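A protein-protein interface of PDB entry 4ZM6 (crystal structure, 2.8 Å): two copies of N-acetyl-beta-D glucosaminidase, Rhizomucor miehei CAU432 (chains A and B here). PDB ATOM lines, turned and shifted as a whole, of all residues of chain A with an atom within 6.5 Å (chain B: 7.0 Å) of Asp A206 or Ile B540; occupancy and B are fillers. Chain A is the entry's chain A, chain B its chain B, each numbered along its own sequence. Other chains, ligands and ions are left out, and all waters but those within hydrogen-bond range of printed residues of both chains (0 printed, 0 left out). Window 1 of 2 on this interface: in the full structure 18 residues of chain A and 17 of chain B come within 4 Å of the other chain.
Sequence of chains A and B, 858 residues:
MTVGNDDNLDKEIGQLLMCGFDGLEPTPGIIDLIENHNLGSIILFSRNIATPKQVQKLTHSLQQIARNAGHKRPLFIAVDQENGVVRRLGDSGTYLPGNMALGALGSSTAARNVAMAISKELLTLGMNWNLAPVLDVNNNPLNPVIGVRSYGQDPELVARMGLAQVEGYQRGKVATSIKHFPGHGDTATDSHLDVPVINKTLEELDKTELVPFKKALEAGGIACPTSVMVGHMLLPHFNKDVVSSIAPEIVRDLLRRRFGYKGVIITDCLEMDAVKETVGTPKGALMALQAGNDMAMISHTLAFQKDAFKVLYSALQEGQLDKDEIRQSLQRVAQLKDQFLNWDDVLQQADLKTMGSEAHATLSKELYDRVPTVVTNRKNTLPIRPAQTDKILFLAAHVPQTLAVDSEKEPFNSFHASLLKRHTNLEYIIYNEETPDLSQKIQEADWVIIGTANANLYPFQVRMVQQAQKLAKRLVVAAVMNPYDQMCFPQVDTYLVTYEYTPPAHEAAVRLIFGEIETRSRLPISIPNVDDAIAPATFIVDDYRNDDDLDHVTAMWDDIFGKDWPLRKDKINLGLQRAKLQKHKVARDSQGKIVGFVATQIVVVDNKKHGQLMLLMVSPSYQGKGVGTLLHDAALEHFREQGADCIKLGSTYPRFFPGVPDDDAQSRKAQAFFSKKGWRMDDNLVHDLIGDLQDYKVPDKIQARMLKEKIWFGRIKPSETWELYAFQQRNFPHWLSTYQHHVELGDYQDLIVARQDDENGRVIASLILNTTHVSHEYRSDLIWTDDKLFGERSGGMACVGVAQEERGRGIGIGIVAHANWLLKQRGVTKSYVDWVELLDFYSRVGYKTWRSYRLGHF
The side-chain carboxylate of Asp B542 lies within salt-bridge range of the guanidinium group of Arg A258, at 2.8 Å.
The side-chain carboxylate of Glu A203 sits at hydrogen-bond distance from the side-chain hydroxyl of Thr B538, 3.0 Å away.
The backbone carbonyl oxygen (O) of Asp B542 lies within hydrogen-bond range of the backbone NH (N) of Val B586 (3.0 Å).
The backbone carbonyl oxygen (O) of Ile B540 sits at hydrogen-bond distance from the backbone NH (N) of Arg B588.
The side-chain carboxylate of Asp A206 is in salt-bridge range of the guanidinium group of Arg A258.
The guanidinium group (NH1) of Arg B588 is in hydrogen-bond range of the backbone carbonyl oxygen (O) of Gly B592.
The side-chain carboxylate of Asp B542 lies within salt-bridge range of the guanidinium group of Arg B588 (3.8 Å).
Leu A202 touches Ile B540 (CD1 to CG2, 3.9 Å).
CG1 of Ile B540 touches OD2 of Asp A206, at 3.8 Å.
NE of Arg A258 touches CG2 of Ile B540, at 3.8 Å.
Arg A258 touches Arg B588 (O to NH2, 3.8 Å).
Of chain B, only Ile B540 (3.8 Å) comes within 4 Å of Asp A206.
Of chain A, only Leu A202 (3.9 Å), Asp A206 (3.8 Å) and Arg A258 (3.8 Å) come within 4 Å of Ile B540.
Of the printed residues of chain B, Glu A203 touches Thr B538.
Printed residues of chain B within 4 Å of Leu A202: Ile B540.
Printed residues of chain A within 4 Å of Thr B538: Glu A203.
Glu A209 touches none of the printed residues of chain B.
Phe B539 touches none of the printed residues of chain A.
Hydrophobic or aromatic side chains of chain A within 4 Å of the printed part of chain B: Leu A202.
Among the printed residues, Asp or Glu carboxylates within 4 Å of a Lys or Arg side-chain nitrogen of the other chain: Arg A258 with Asp B542 (2.8 Å).
No position is printed for both chains.
Of the 6 pairs that touch across the chains among the printed residues, none has its exchanged pair printed and touching as well.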
ATOM      1  N   THR A 201     -16.956  -5.315  -1.848  1.00  0.00           N
ATOM      2  CA  THR A 201     -17.318  -3.910  -2.002  1.00  0.00           C
ATOM      3  C   THR A 201     -16.161  -3.028  -1.550  1.00  0.00           C
ATOM      4  O   THR A 201     -15.209  -3.505  -0.923  1.00  0.00           O
ATOM      5  CB  THR A 201     -18.572  -3.552  -1.172  1.00  0.00           C
ATOM      6  OG1 THR A 201     -18.402  -3.992   0.183  1.00  0.00           O
ATOM      7  CG2 THR A 201     -19.817  -4.203  -1.762  1.00  0.00           C
ATOM      8  N   LEU A 202     -16.255  -1.737  -1.863  1.00  0.00           N
ATOM      9  CA  LEU A 202     -15.218  -0.781  -1.485  1.00  0.00           C
ATOM     10  C   LEU A 202     -15.039  -0.742   0.037  1.00  0.00           C
ATOM     11  O   LEU A 202     -13.916  -0.612   0.524  1.00  0.00           O
ATOM     12  CB  LEU A 202     -15.541   0.626  -2.007  1.00  0.00           C
ATOM     13  CG  LEU A 202     -14.407   1.494  -2.577  1.00  0.00           C
ATOM     14  CD1 LEU A 202     -14.717   2.965  -2.332  1.00  0.00           C
ATOM     15  CD2 LEU A 202     -13.030   1.159  -2.020  1.00  0.00           C
ATOM     16  N   GLU A 203     -16.140  -0.878   0.779  1.00  0.00           N
ATOM     17  CA  GLU A 203     -16.091  -0.861   2.245  1.00  0.00           C
ATOM     18  C   GLU A 203     -15.316  -2.057   2.796  1.00  0.00           C
ATOM     19  O   GLU A 203     -14.532  -1.912   3.737  1.00  0.00           O
ATOM     20  CB  GLU A 203     -17.496  -0.825   2.856  1.00  0.00           C
ATOM     21  CG  GLU A 203     -18.196   0.523   2.739  1.00  0.00           C
ATOM     22  CD  GLU A 203     -18.830   0.771   1.375  1.00  0.00           C
ATOM     23  OE1 GLU A 203     -19.330   1.896   1.161  1.00  0.00           O
ATOM     24  OE2 GLU A 203     -18.837  -0.145   0.518  1.00  0.00           O
ATOM     25  N   GLU A 204     -15.542  -3.233   2.212  1.00  0.00           N
ATOM     26  CA  GLU A 204     -14.779  -4.429   2.578  1.00  0.00           C
ATOM     27  C   GLU A 204     -13.306  -4.250   2.209  1.00  0.00           C
ATOM     28  O   GLU A 204     -12.417  -4.564   3.001  1.00  0.00           O
ATOM     29  CB  GLU A 204     -15.328  -5.669   1.876  1.00  0.00           C
ATOM     30  CG  GLU A 204     -16.728  -6.084   2.295  1.00  0.00           C
ATOM     31  CD  GLU A 204     -17.227  -7.284   1.503  1.00  0.00           C
ATOM     32  OE1 GLU A 204     -16.910  -8.433   1.888  1.00  0.00           O
ATOM     33  OE2 GLU A 204     -17.933  -7.078   0.491  1.00  0.00           O
ATOM     34  N   LEU A 205     -13.057  -3.737   1.005  1.00  0.00           N
ATOM     35  CA  LEU A 205     -11.691  -3.500   0.531  1.00  0.00           C
ATOM     36  C   LEU A 205     -10.918  -2.525   1.419  1.00  0.00           C
ATOM     37  O   LEU A 205      -9.723  -2.708   1.648  1.00  0.00           O
ATOM     38  CB  LEU A 205     -11.697  -2.998  -0.919  1.00  0.00           C
ATOM     39  CG  LEU A 205     -11.995  -4.074  -1.969  1.00  0.00           C
ATOM     40  CD1 LEU A 205     -12.308  -3.446  -3.316  1.00  0.00           C
ATOM     41  CD2 LEU A 205     -10.837  -5.055  -2.098  1.00  0.00           C
ATOM     42  N   ASP A 206     -11.602  -1.498   1.915  1.00  0.00           N
ATOM     43  CA  ASP A 206     -10.980  -0.517   2.807  1.00  0.00           C
ATOM     44  C   ASP A 206     -10.486  -1.129   4.115  1.00  0.00           C
ATOM     45  O   ASP A 206      -9.493  -0.667   4.676  1.00  0.00           O
ATOM     46  CB  ASP A 206     -11.948   0.635   3.116  1.00  0.00           C
ATOM     47  CG  ASP A 206     -12.014   1.665   1.998  1.00  0.00           C
ATOM     48  OD1 ASP A 206     -11.068   1.743   1.182  1.00  0.00           O
ATOM     49  OD2 ASP A 206     -13.015   2.414   1.943  1.00  0.00           O
ATOM     50  N   LYS A 207     -11.175  -2.158   4.601  1.00  0.00           N
ATOM     51  CA  LYS A 207     -10.832  -2.759   5.891  1.00  0.00           C
ATOM     52  C   LYS A 207      -9.562  -3.628   5.838  1.00  0.00           C
ATOM     53  O   LYS A 207      -8.881  -3.763   6.854  1.00  0.00           O
ATOM     54  CB  LYS A 207     -12.018  -3.553   6.460  1.00  0.00           C
ATOM     55  N   THR A 208      -9.233  -4.206   4.677  1.00  0.00           N
ATOM     56  CA  THR A 208      -8.039  -5.065   4.569  1.00  0.00           C
ATOM     57  C   THR A 208      -7.184  -4.803   3.323  1.00  0.00           C
ATOM     58  O   THR A 208      -6.043  -4.355   3.437  1.00  0.00           O
ATOM     59  CB  THR A 208      -8.395  -6.577   4.629  1.00  0.00           C
ATOM     60  OG1 THR A 208      -9.044  -6.980   3.419  1.00  0.00           O
ATOM     61  CG2 THR A 208      -9.304  -6.902   5.821  1.00  0.00           C
ATOM     62  N   GLU A 209      -7.725  -5.098   2.144  1.00  0.00           N
ATOM     63  CA  GLU A 209      -6.942  -5.070   0.901  1.00  0.00           C
ATOM     64  C   GLU A 209      -6.197  -3.755   0.685  1.00  0.00           C
ATOM     65  O   GLU A 209      -5.008  -3.756   0.375  1.00  0.00           O
ATOM     66  CB  GLU A 209      -7.827  -5.346  -0.322  1.00  0.00           C
ATOM     67  CG  GLU A 209      -7.905  -6.806  -0.750  1.00  0.00           C
ATOM     68  CD  GLU A 209      -8.857  -7.645   0.091  1.00  0.00           C
ATOM     69  OE1 GLU A 209      -9.484  -7.105   1.021  1.00  0.00           O
ATOM     70  OE2 GLU A 209      -8.986  -8.855  -0.188  1.00  0.00           O
ATOM     71  N   LEU A 210      -6.906  -2.643   0.853  1.00  0.00           N
ATOM     72  CA  LEU A 210      -6.367  -1.329   0.517  1.00  0.00           C
ATOM     73  C   LEU A 210      -5.595  -0.659   1.662  1.00  0.00           C
ATOM     74  O   LEU A 210      -4.948   0.367   1.443  1.00  0.00           O
ATOM     75  CB  LEU A 210      -7.493  -0.414   0.027  1.00  0.00           C
ATOM     76  CG  LEU A 210      -8.142  -0.826  -1.296  1.00  0.00           C
ATOM     77  CD1 LEU A 210      -9.475  -0.124  -1.498  1.00  0.00           C
ATOM     78  CD2 LEU A 210      -7.217  -0.543  -2.472  1.00  0.00           C
ATOM     79  N   VAL A 211      -5.642  -1.227   2.866  1.00  0.00           N
ATOM     80  CA  VAL A 211      -4.951  -0.620   4.005  1.00  0.00           C
ATOM     81  C   VAL A 211      -3.484  -0.344   3.681  1.00  0.00           C
ATOM     82  O   VAL A 211      -3.046   0.799   3.797  1.00  0.00           O
ATOM     83  CB  VAL A 211      -5.068  -1.452   5.303  1.00  0.00           C
ATOM     84  CG1 VAL A 211      -4.129  -0.920   6.382  1.00  0.00           C
ATOM     85  CG2 VAL A 211      -6.502  -1.446   5.812  1.00  0.00           C
ATOM     86  N   ARG A 258     -10.297   8.793  -6.450  1.00  0.00           N
ATOM     87  CA  ARG A 258     -10.509   8.618  -5.003  1.00  0.00           C
ATOM     88  C   ARG A 258      -9.226   8.827  -4.187  1.00  0.00           C
ATOM     89  O   ARG A 258      -9.164   9.727  -3.352  1.00  0.00           O
ATOM     90  CB  ARG A 258     -11.097   7.232  -4.709  1.00  0.00           C
ATOM     91  CG  ARG A 258     -10.987   6.773  -3.256  1.00  0.00           C
ATOM     92  CD  ARG A 258     -12.341   6.497  -2.626  1.00  0.00           C
ATOM     93  NE  ARG A 258     -12.243   6.227  -1.188  1.00  0.00           N
ATOM     94  CZ  ARG A 258     -11.801   5.091  -0.642  1.00  0.00           C
ATOM     95  NH1 ARG A 258     -11.382   4.079  -1.394  1.00  0.00           N
ATOM     96  NH2 ARG A 258     -11.772   4.969   0.678  1.00  0.00           N
ATOM     97  N   PHE A 259      -8.215   7.993  -4.422  1.00  0.00           N
ATOM     98  CA  PHE A 259      -6.962   8.081  -3.673  1.00  0.00           C
ATOM     99  C   PHE A 259      -6.098   9.276  -4.070  1.00  0.00           C
ATOM    100  O   PHE A 259      -5.228   9.684  -3.302  1.00  0.00           O
ATOM    101  CB  PHE A 259      -6.155   6.784  -3.789  1.00  0.00           C
ATOM    102  CG  PHE A 259      -6.686   5.669  -2.929  1.00  0.00           C
ATOM    103  CD1 PHE A 259      -6.717   5.799  -1.543  1.00  0.00           C
ATOM    104  CD2 PHE A 259      -7.158   4.492  -3.497  1.00  0.00           C
ATOM    105  CE1 PHE A 259      -7.211   4.782  -0.745  1.00  0.00           C
ATOM    106  CE2 PHE A 259      -7.650   3.470  -2.703  1.00  0.00           C
ATOM    107  CZ  PHE A 259      -7.678   3.615  -1.327  1.00  0.00           C
ATOM    108  N   THR B 538     -23.615   2.708  -2.176  1.00  0.00           N
ATOM    109  CA  THR B 538     -23.018   3.283  -0.976  1.00  0.00           C
ATOM    110  C   THR B 538     -22.100   4.453  -1.271  1.00  0.00           C
ATOM    111  O   THR B 538     -21.540   4.573  -2.361  1.00  0.00           O
ATOM    112  CB  THR B 538     -22.202   2.246  -0.185  1.00  0.00           C
ATOM    113  OG1 THR B 538     -21.319   1.550  -1.076  1.00  0.00           O
ATOM    114  CG2 THR B 538     -23.124   1.255   0.524  1.00  0.00           C
ATOM    115  N   PHE B 539     -21.958   5.300  -0.256  1.00  0.00           N
ATOM    116  CA  PHE B 539     -21.098   6.465  -0.299  1.00  0.00           C
ATOM    117  C   PHE B 539     -20.088   6.347   0.828  1.00  0.00           C
ATOM    118  O   PHE B 539     -20.455   6.040   1.962  1.00  0.00           O
ATOM    119  CB  PHE B 539     -21.931   7.732  -0.124  1.00  0.00           C
ATOM    120  CG  PHE B 539     -23.003   7.892  -1.161  1.00  0.00           C
ATOM    121  CD1 PHE B 539     -22.720   8.492  -2.380  1.00  0.00           C
ATOM    122  CD2 PHE B 539     -24.288   7.422  -0.929  1.00  0.00           C
ATOM    123  CE1 PHE B 539     -23.702   8.632  -3.346  1.00  0.00           C
ATOM    124  CE2 PHE B 539     -25.270   7.557  -1.889  1.00  0.00           C
ATOM    125  CZ  PHE B 539     -24.979   8.166  -3.101  1.00  0.00           C
ATOM    126  N   ILE B 540     -18.818   6.584   0.512  1.00  0.00           N
ATOM    127  CA  ILE B 540     -17.750   6.483   1.502  1.00  0.00           C
ATOM    128  C   ILE B 540     -17.172   7.876   1.789  1.00  0.00           C
ATOM    129  O   ILE B 540     -17.140   8.735   0.903  1.00  0.00           O
ATOM    130  CB  ILE B 540     -16.663   5.474   1.054  1.00  0.00           C
ATOM    131  CG1 ILE B 540     -15.749   5.097   2.223  1.00  0.00           C
ATOM    132  CG2 ILE B 540     -15.837   6.014  -0.109  1.00  0.00           C
ATOM    133  CD1 ILE B 540     -16.459   4.415   3.376  1.00  0.00           C
ATOM    134  N   VAL B 541     -16.738   8.087   3.034  1.00  0.00           N
ATOM    135  CA  VAL B 541     -16.253   9.389   3.504  1.00  0.00           C
ATOM    136  C   VAL B 541     -14.734   9.394   3.727  1.00  0.00           C
ATOM    137  O   VAL B 541     -14.227   8.628   4.542  1.00  0.00           O
ATOM    138  CB  VAL B 541     -16.955   9.778   4.825  1.00  0.00           C
ATOM    139  CG1 VAL B 541     -16.313  11.009   5.450  1.00  0.00           C
ATOM    140  CG2 VAL B 541     -18.440  10.014   4.589  1.00  0.00           C
ATOM    141  N   ASP B 542     -14.025  10.268   3.008  1.00  0.00           N
ATOM    142  CA  ASP B 542     -12.575  10.466   3.181  1.00  0.00           C
ATOM    143  C   ASP B 542     -12.256  11.865   3.709  1.00  0.00           C
ATOM    144  O   ASP B 542     -13.087  12.772   3.662  1.00  0.00           O
ATOM    145  CB  ASP B 542     -11.838  10.291   1.846  1.00  0.00           C
ATOM    146  CG  ASP B 542     -11.793   8.855   1.380  1.00  0.00           C
ATOM    147  OD1 ASP B 542     -11.320   7.992   2.152  1.00  0.00           O
ATOM    148  OD2 ASP B 542     -12.216   8.596   0.230  1.00  0.00           O
ATOM    149  N   VAL B 586     -15.058  14.776   2.726  1.00  0.00           N
ATOM    150  CA  VAL B 586     -15.892  14.719   1.525  1.00  0.00           C
ATOM    151  C   VAL B 586     -16.541  13.349   1.447  1.00  0.00           C
ATOM    152  O   VAL B 586     -15.995  12.370   1.958  1.00  0.00           O
ATOM    153  CB  VAL B 586     -15.103  14.968   0.217  1.00  0.00           C
ATOM    154  CG1 VAL B 586     -14.458  16.346   0.233  1.00  0.00           C
ATOM    155  CG2 VAL B 586     -14.068  13.872  -0.032  1.00  0.00           C
ATOM    156  N   ALA B 587     -17.707  13.290   0.811  1.00  0.00           N
ATOM    157  CA  ALA B 587     -18.373  12.024   0.536  1.00  0.00           C
ATOM    158  C   ALA B 587     -18.300  11.740  -0.961  1.00  0.00           C
ATOM    159  O   ALA B 587     -18.651  12.590  -1.777  1.00  0.00           O
ATOM    160  CB  ALA B 587     -19.819  12.073   1.002  1.00  0.00           C
ATOM    161  N   ARG B 588     -17.823  10.550  -1.314  1.00  0.00           N
ATOM    162  CA  ARG B 588     -17.756  10.123  -2.708  1.00  0.00           C
ATOM    163  C   ARG B 588     -18.736   8.986  -2.953  1.00  0.00           C
ATOM    164  O   ARG B 588     -19.145   8.305  -2.013  1.00  0.00           O
ATOM    165  CB  ARG B 588     -16.345   9.650  -3.053  1.00  0.00           C
ATOM    166  CG  ARG B 588     -15.274  10.716  -2.919  1.00  0.00           C
ATOM    167  CD  ARG B 588     -13.889  10.137  -3.165  1.00  0.00           C
ATOM    168  NE  ARG B 588     -12.812  11.006  -2.678  1.00  0.00           N
ATOM    169  CZ  ARG B 588     -12.295  12.045  -3.337  1.00  0.00           C
ATOM    170  NH1 ARG B 588     -12.744  12.396  -4.540  1.00  0.00           N
ATOM    171  NH2 ARG B 588     -11.314  12.747  -2.781  1.00  0.00           N
ATOM    172  N   ASP B 589     -19.113   8.789  -4.213  1.00  0.00           N
ATOM    173  CA  ASP B 589     -19.831   7.577  -4.615  1.00  0.00           C
ATOM    174  C   ASP B 589     -18.805   6.474  -4.913  1.00  0.00           C
ATOM    175  O   ASP B 589     -17.611   6.656  -4.665  1.00  0.00           O
ATOM    176  CB  ASP B 589     -20.784   7.845  -5.797  1.00  0.00           C
ATOM    177  CG  ASP B 589     -20.075   8.363  -7.044  1.00  0.00           C
ATOM    178  OD1 ASP B 589     -18.899   8.008  -7.277  1.00  0.00           O
ATOM    179  OD2 ASP B 589     -20.712   9.124  -7.805  1.00  0.00           O
ATOM    180  N   SER B 590     -19.263   5.332  -5.421  1.00  0.00           N
ATOM    181  CA  SER B 590     -18.367   4.209  -5.735  1.00  0.00           C
ATOM    182  C   SER B 590     -17.281   4.570  -6.757  1.00  0.00           C
ATOM    183  O   SER B 590     -16.189   3.993  -6.740  1.00  0.00           O
ATOM    184  CB  SER B 590     -19.176   3.018  -6.250  1.00  0.00           C
ATOM    185  OG  SER B 590     -19.919   3.375  -7.401  1.00  0.00           O
ATOM    186  N   GLY B 592     -15.739   7.469  -6.984  1.00  0.00           N
ATOM    187  CA  GLY B 592     -14.844   8.505  -6.463  1.00  0.00           C
ATOM    188  C   GLY B 592     -15.285   9.939  -6.719  1.00  0.00           C
ATOM    189  O   GLY B 592     -14.543  10.877  -6.421  1.00  0.00           O
ATOM    190  N   VAL B 595     -19.794  14.028  -3.787  1.00  0.00           N
ATOM    191  CA  VAL B 595     -21.234  14.289  -3.733  1.00  0.00           C
ATOM    192  C   VAL B 595     -21.693  14.989  -2.455  1.00  0.00           C
ATOM    193  O   VAL B 595     -22.881  15.271  -2.296  1.00  0.00           O
ATOM    194  CB  VAL B 595     -22.035  12.975  -3.874  1.00  0.00           C
ATOM    195  CG1 VAL B 595     -21.803  12.366  -5.249  1.00  0.00           C
ATOM    196  CG2 VAL B 595     -21.668  11.979  -2.776  1.00  0.00           C
ATOM    197  N   LEU B 630     -24.336  10.640   6.882  1.00  0.00           N
ATOM    198  CA  LEU B 630     -22.986  10.075   6.911  1.00  0.00           C
ATOM    199  C   LEU B 630     -21.945  11.122   7.292  1.00  0.00           C
ATOM    200  O   LEU B 630     -21.158  10.910   8.217  1.00  0.00           O
ATOM    201  CB  LEU B 630     -22.619   9.455   5.558  1.00  0.00           C
ATOM    202  CG  LEU B 630     -22.694   7.929   5.441  1.00  0.00           C
ATOM    203  CD1 LEU B 630     -24.045   7.357   5.847  1.00  0.00           C
ATOM    204  CD2 LEU B 630     -22.368   7.532   4.010  1.00  0.00           C
ATOM    205  N   LEU B 631     -21.948  12.243   6.573  1.00  0.00           N
ATOM    206  CA  LEU B 631     -21.011  13.333   6.837  1.00  0.00           C
ATOM    207  C   LEU B 631     -21.256  13.915   8.216  1.00  0.00           C
ATOM    208  O   LEU B 631     -20.321  14.130   8.978  1.00  0.00           O
ATOM    209  CB  LEU B 631     -21.146  14.435   5.785  1.00  0.00           C
ATOM    210  CG  LEU B 631     -20.701  14.050   4.372  1.00  0.00           C
ATOM    211  CD1 LEU B 631     -21.187  15.073   3.359  1.00  0.00           C
ATOM    212  CD2 LEU B 631     -19.189  13.896   4.292  1.00  0.00           C
